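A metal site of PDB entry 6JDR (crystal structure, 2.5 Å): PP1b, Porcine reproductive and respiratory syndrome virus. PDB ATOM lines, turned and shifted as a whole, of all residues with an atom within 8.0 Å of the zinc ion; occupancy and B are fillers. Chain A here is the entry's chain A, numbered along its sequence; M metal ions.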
ATOM      1  N   TYR A   9      27.709 -18.359  24.023  1.00  0.00           N
ATOM      2  CA  TYR A   9      29.144 -18.468  23.751  1.00  0.00           C
ATOM      3  C   TYR A   9      29.837 -17.119  23.909  1.00  0.00           C
ATOM      4  O   TYR A   9      30.749 -16.967  24.743  1.00  0.00           O
ATOM      5  CB  TYR A   9      29.401 -18.974  22.337  1.00  0.00           C
ATOM      6  CG  TYR A   9      29.005 -20.410  22.065  1.00  0.00           C
ATOM      7  CD1 TYR A   9      29.684 -21.466  22.676  1.00  0.00           C
ATOM      8  CD2 TYR A   9      27.975 -20.724  21.191  1.00  0.00           C
ATOM      9  CE1 TYR A   9      29.339 -22.779  22.427  1.00  0.00           C
ATOM     10  CE2 TYR A   9      27.628 -22.032  20.925  1.00  0.00           C
ATOM     11  CZ  TYR A   9      28.311 -23.062  21.551  1.00  0.00           C
ATOM     12  OH  TYR A   9      27.966 -24.375  21.302  1.00  0.00           O
ATOM     13  N   ALA A  17      18.361 -20.305  19.039  1.00  0.00           N
ATOM     14  CA  ALA A  17      18.732 -21.117  20.191  1.00  0.00           C
ATOM     15  C   ALA A  17      18.917 -22.582  19.804  1.00  0.00           C
ATOM     16  O   ALA A  17      18.334 -23.055  18.825  1.00  0.00           O
ATOM     17  CB  ALA A  17      17.666 -21.006  21.270  1.00  0.00           C
ATOM     18  N   THR A  18      19.746 -23.287  20.579  1.00  0.00           N
ATOM     19  CA  THR A  18      19.926 -24.729  20.391  1.00  0.00           C
ATOM     20  C   THR A  18      18.750 -25.454  21.016  1.00  0.00           C
ATOM     21  O   THR A  18      18.072 -24.909  21.884  1.00  0.00           O
ATOM     22  CB  THR A  18      21.238 -25.255  21.039  1.00  0.00           C
ATOM     23  OG1 THR A  18      21.148 -25.176  22.466  1.00  0.00           O
ATOM     24  CG2 THR A  18      22.437 -24.446  20.552  1.00  0.00           C
ATOM     25  N   ALA A  19      18.519 -26.683  20.564  1.00  0.00           N
ATOM     26  CA  ALA A  19      17.467 -27.513  21.135  1.00  0.00           C
ATOM     27  C   ALA A  19      17.695 -27.809  22.616  1.00  0.00           C
ATOM     28  O   ALA A  19      16.759 -28.071  23.356  1.00  0.00           O
ATOM     29  CB  ALA A  19      17.339 -28.813  20.349  1.00  0.00           C
ATOM     30  N   CYS A  20      18.964 -27.760  23.038  1.00  0.00           N
ATOM     31  CA  CYS A  20      19.324 -27.986  24.445  1.00  0.00           C
ATOM     32  C   CYS A  20      19.302 -26.708  25.299  1.00  0.00           C
ATOM     33  O   CYS A  20      19.798 -26.718  26.430  1.00  0.00           O
ATOM     34  CB  CYS A  20      20.689 -28.667  24.525  1.00  0.00           C
ATOM     35  SG  CYS A  20      22.083 -27.600  24.101  1.00  0.00           S
ATOM     36  N   GLY A  21      18.740 -25.624  24.780  1.00  0.00           N
ATOM     37  CA  GLY A  21      18.447 -24.426  25.582  1.00  0.00           C
ATOM     38  C   GLY A  21      19.489 -23.315  25.579  1.00  0.00           C
ATOM     39  O   GLY A  21      19.379 -22.374  26.353  1.00  0.00           O
ATOM     40  N   LEU A  22      20.480 -23.410  24.688  1.00  0.00           N
ATOM     41  CA  LEU A  22      21.533 -22.392  24.608  1.00  0.00           C
ATOM     42  C   LEU A  22      21.167 -21.324  23.575  1.00  0.00           C
ATOM     43  O   LEU A  22      20.953 -21.648  22.407  1.00  0.00           O
ATOM     44  CB  LEU A  22      22.866 -23.050  24.221  1.00  0.00           C
ATOM     45  CG  LEU A  22      24.113 -22.175  24.360  1.00  0.00           C
ATOM     46  CD1 LEU A  22      24.473 -21.942  25.822  1.00  0.00           C
ATOM     47  CD2 LEU A  22      25.288 -22.812  23.632  1.00  0.00           C
ATOM     48  N   HIS A  32      27.611 -25.806  16.680  1.00  0.00           N
ATOM     49  CA  HIS A  32      27.026 -26.524  17.811  1.00  0.00           C
ATOM     50  C   HIS A  32      26.575 -27.897  17.346  1.00  0.00           C
ATOM     51  O   HIS A  32      25.422 -28.091  16.962  1.00  0.00           O
ATOM     52  CB  HIS A  32      25.868 -25.724  18.390  1.00  0.00           C
ATOM     53  CG  HIS A  32      25.321 -26.277  19.666  1.00  0.00           C
ATOM     54  ND1 HIS A  32      25.779 -25.884  20.905  1.00  0.00           N
ATOM     55  CD2 HIS A  32      24.336 -27.177  19.895  1.00  0.00           C
ATOM     56  CE1 HIS A  32      25.109 -26.534  21.843  1.00  0.00           C
ATOM     57  NE2 HIS A  32      24.222 -27.313  21.250  1.00  0.00           N
ATOM     58  N   GLN A  33      27.485 -28.859  17.397  1.00  0.00           N
ATOM     59  CA  GLN A  33      27.232 -30.199  16.867  1.00  0.00           C
ATOM     60  C   GLN A  33      26.457 -31.080  17.850  1.00  0.00           C
ATOM     61  O   GLN A  33      26.019 -32.171  17.482  1.00  0.00           O
ATOM     62  CB  GLN A  33      28.551 -30.864  16.467  1.00  0.00           C
ATOM     63  CG  GLN A  33      29.331 -30.067  15.441  1.00  0.00           C
ATOM     64  CD  GLN A  33      30.552 -30.797  14.915  1.00  0.00           C
ATOM     65  OE1 GLN A  33      31.233 -31.502  15.648  1.00  0.00           O
ATOM     66  NE2 GLN A  33      30.838 -30.626  13.634  1.00  0.00           N
ATOM     67  N   HIS A  34      26.310 -30.613  19.081  1.00  0.00           N
ATOM     68  CA  HIS A  34      25.599 -31.345  20.139  1.00  0.00           C
ATOM     69  C   HIS A  34      24.152 -31.683  19.795  1.00  0.00           C
ATOM     70  O   HIS A  34      23.683 -32.782  20.068  1.00  0.00           O
ATOM     71  CB  HIS A  34      25.650 -30.524  21.428  1.00  0.00           C
ATOM     72  CG  HIS A  34      24.893 -31.126  22.568  1.00  0.00           C
ATOM     73  ND1 HIS A  34      23.756 -30.539  23.089  1.00  0.00           N
ATOM     74  CD2 HIS A  34      25.103 -32.247  23.296  1.00  0.00           C
ATOM     75  CE1 HIS A  34      23.295 -31.281  24.078  1.00  0.00           C
ATOM     76  NE2 HIS A  34      24.096 -32.323  24.227  1.00  0.00           N
ATOM     77  N   CYS A  35      23.442 -30.736  19.192  1.00  0.00           N
ATOM     78  CA  CYS A  35      22.025 -30.906  18.903  1.00  0.00           C
ATOM     79  C   CYS A  35      21.568 -29.905  17.846  1.00  0.00           C
ATOM     80  O   CYS A  35      22.310 -28.974  17.526  1.00  0.00           O
ATOM     81  CB  CYS A  35      21.199 -30.763  20.188  1.00  0.00           C
ATOM     82  SG  CYS A  35      21.218 -29.104  20.898  1.00  0.00           S
ATOM     83  N   PRO A  36      20.359 -30.096  17.287  1.00  0.00           N
ATOM     84  CA  PRO A  36      19.900 -29.203  16.224  1.00  0.00           C
ATOM     85  C   PRO A  36      19.778 -27.725  16.613  1.00  0.00           C
ATOM     86  O   PRO A  36      19.419 -27.399  17.756  1.00  0.00           O
ATOM     87  CB  PRO A  36      18.506 -29.753  15.879  1.00  0.00           C
ATOM     88  CG  PRO A  36      18.561 -31.188  16.272  1.00  0.00           C
ATOM     89  CD  PRO A  36      19.429 -31.224  17.490  1.00  0.00           C
ATOM     90  N   VAL A  37      20.081 -26.858  15.659  1.00  0.00           N
ATOM     91  CA  VAL A  37      19.842 -25.432  15.794  1.00  0.00           C
ATOM     92  C   VAL A  37      18.960 -24.984  14.622  1.00  0.00           C
ATOM     93  O   VAL A  37      19.428 -24.883  13.489  1.00  0.00           O
ATOM     94  CB  VAL A  37      21.156 -24.627  15.782  1.00  0.00           C
ATOM     95  CG1 VAL A  37      20.886 -23.147  16.020  1.00  0.00           C
ATOM     96  CG2 VAL A  37      22.113 -25.179  16.827  1.00  0.00           C
ATOM     97  N   LEU A  64      32.808 -25.537  26.224  1.00  0.00           N
ATOM     98  CA  LEU A  64      31.438 -26.012  26.401  1.00  0.00           C
ATOM     99  C   LEU A  64      31.118 -27.154  25.450  1.00  0.00           C
ATOM    100  O   LEU A  64      30.449 -28.107  25.827  1.00  0.00           O
ATOM    101  CB  LEU A  64      30.439 -24.877  26.157  1.00  0.00           C
ATOM    102  CG  LEU A  64      28.957 -25.226  26.301  1.00  0.00           C
ATOM    103  CD1 LEU A  64      28.628 -25.651  27.727  1.00  0.00           C
ATOM    104  CD2 LEU A  64      28.089 -24.048  25.887  1.00  0.00           C
ATOM    105  N   ASP A  65      31.606 -27.042  24.226  1.00  0.00           N
ATOM    106  CA  ASP A  65      31.294 -28.023  23.200  1.00  0.00           C
ATOM    107  C   ASP A  65      31.967 -29.353  23.514  1.00  0.00           C
ATOM    108  O   ASP A  65      31.400 -30.411  23.242  1.00  0.00           O
ATOM    109  CB  ASP A  65      31.722 -27.488  21.829  1.00  0.00           C
ATOM    110  CG  ASP A  65      31.059 -26.172  21.497  1.00  0.00           C
ATOM    111  OD1 ASP A  65      29.813 -26.105  21.593  1.00  0.00           O
ATOM    112  OD2 ASP A  65      31.777 -25.197  21.164  1.00  0.00           O
ATOM    113  N   LEU A  68      29.974 -30.929  26.297  1.00  0.00           N
ATOM    114  CA  LEU A  68      28.706 -31.444  25.792  1.00  0.00           C
ATOM    115  C   LEU A  68      28.809 -32.775  25.031  1.00  0.00           C
ATOM    116  O   LEU A  68      27.798 -33.408  24.790  1.00  0.00           O
ATOM    117  CB  LEU A  68      27.989 -30.402  24.928  1.00  0.00           C
ATOM    118  CG  LEU A  68      27.379 -29.196  25.654  1.00  0.00           C
ATOM    119  CD1 LEU A  68      26.873 -28.181  24.646  1.00  0.00           C
ATOM    120  CD2 LEU A  68      26.279 -29.612  26.609  1.00  0.00           C
ATOM    121  N   VAL A  71      27.142 -35.299  27.008  1.00  0.00           N
ATOM    122  CA  VAL A  71      25.773 -34.957  27.389  1.00  0.00           C
ATOM    123  C   VAL A  71      24.816 -35.341  26.247  1.00  0.00           C
ATOM    124  O   VAL A  71      24.727 -34.628  25.256  1.00  0.00           O
ATOM    125  CB  VAL A  71      25.649 -33.453  27.720  1.00  0.00           C
ATOM    126  CG1 VAL A  71      24.260 -33.133  28.263  1.00  0.00           C
ATOM    127  CG2 VAL A  71      26.714 -33.042  28.728  1.00  0.00           C
ATOM    128  N   PRO A  72      24.123 -36.495  26.372  1.00  0.00           N
ATOM    129  CA  PRO A  72      23.211 -36.972  25.320  1.00  0.00           C
ATOM    130  C   PRO A  72      22.015 -36.058  25.075  1.00  0.00           C
ATOM    131  O   PRO A  72      21.347 -35.659  26.021  1.00  0.00           O
ATOM    132  CB  PRO A  72      22.698 -38.313  25.861  1.00  0.00           C
ATOM    133  CG  PRO A  72      23.643 -38.711  26.936  1.00  0.00           C
ATOM    134  CD  PRO A  72      24.230 -37.457  27.483  1.00  0.00           C
ATOM    135  N   TYR A  73      21.756 -35.741  23.810  1.00  0.00           N
ATOM    136  CA  TYR A  73      20.552 -35.032  23.439  1.00  0.00           C
ATOM    137  C   TYR A  73      19.439 -36.048  23.189  1.00  0.00           C
ATOM    138  O   TYR A  73      19.570 -36.907  22.317  1.00  0.00           O
ATOM    139  CB  TYR A  73      20.763 -34.169  22.194  1.00  0.00           C
ATOM    140  CG  TYR A  73      19.476 -33.572  21.672  1.00  0.00           C
ATOM    141  CD1 TYR A  73      18.732 -32.702  22.465  1.00  0.00           C
ATOM    142  CD2 TYR A  73      18.996 -33.893  20.406  1.00  0.00           C
ATOM    143  CE1 TYR A  73      17.546 -32.164  22.002  1.00  0.00           C
ATOM    144  CE2 TYR A  73      17.803 -33.357  19.936  1.00  0.00           C
ATOM    145  CZ  TYR A  73      17.090 -32.497  20.746  1.00  0.00           C
ATOM    146  OH  TYR A  73      15.905 -31.955  20.297  1.00  0.00           O
ATOM    147  N   LEU A 126      15.108 -27.982  25.753  1.00  0.00           N
ATOM    148  CA  LEU A 126      15.502 -28.647  26.996  1.00  0.00           C
ATOM    149  C   LEU A 126      16.165 -27.650  27.936  1.00  0.00           C
ATOM    150  O   LEU A 126      16.683 -26.608  27.494  1.00  0.00           O
ATOM    151  CB  LEU A 126      16.458 -29.803  26.696  1.00  0.00           C
ATOM    152  CG  LEU A 126      15.912 -30.938  25.822  1.00  0.00           C
ATOM    153  CD1 LEU A 126      17.017 -31.893  25.412  1.00  0.00           C
ATOM    154  CD2 LEU A 126      14.816 -31.702  26.551  1.00  0.00           C
ATOM    155  N   THR A 128      18.908 -28.175  29.515  1.00  0.00           N
ATOM    156  CA  THR A 128      20.338 -28.500  29.613  1.00  0.00           C
ATOM    157  C   THR A 128      21.230 -27.265  29.747  1.00  0.00           C
ATOM    158  O   THR A 128      21.981 -27.160  30.722  1.00  0.00           O
ATOM    159  CB  THR A 128      20.819 -29.316  28.406  1.00  0.00           C
ATOM    160  OG1 THR A 128      19.889 -30.370  28.111  1.00  0.00           O
ATOM    161  CG2 THR A 128      22.206 -29.929  28.680  1.00  0.00           C
ATOM    162  N   CYS A 129      21.143 -26.351  28.795  1.00  0.00           N
ATOM    163  CA  CYS A 129      22.004 -25.163  28.782  1.00  0.00           C
ATOM    164  C   CYS A 129      21.226 -23.863  29.015  1.00  0.00           C
ATOM    165  O   CYS A 129      21.676 -22.791  28.617  1.00  0.00           O
ATOM    166  CB  CYS A 129      22.781 -25.089  27.474  1.00  0.00           C
ATOM    167  SG  CYS A 129      23.986 -26.425  27.257  1.00  0.00           S
HETATM  168 ZN    ZN M   1      22.946 -28.691  22.302  1.00  0.00          ZN
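A ring nitrogen (ND1) of His 32 sits at hydrogen-bond distance from the side-chain hydroxyl (OH) of Tyr 9 (2.7 Å).
The backbone carbonyl oxygen of Cys 20 sits at hydrogen-bond distance from the backbone NH of Cys 129 (2.7 Å).
OG1 of Thr 18 sits close to N of Cys 20 (3.4 Å).
N of Ala 19 sits close to SG of Cys 35 (3.6 Å).
A ring nitrogen (NE2) of His 34 lies within hydrogen-bond range of the backbone carbonyl oxygen (O) of Val 71 (2.6 Å).
The side-chain hydroxyl (OG1) of Thr 18 lies within hydrogen-bond range of the backbone NH (N) of Leu 22 (2.9 Å).
The side-chain hydroxyl of Thr 18 lies within hydrogen-bond range of the backbone NH of Gly 21.
Merely in contact with the zinc ion: Thr 18.
Of the 22 residues printed, 5 come within 4 Å of the zinc ion.
The nearest printed residue that does not touch the zinc ion is Leu 68 (4.6 Å).
The zinc ion is bound by NE2 of His 32 (2.2 Å), ND1 of His 34 (2.2 Å), SG of Cys 35 (2.3 Å) and SG of Cys 20 (2.3 Å).
The zinc ion has four donor atoms within binding distance.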
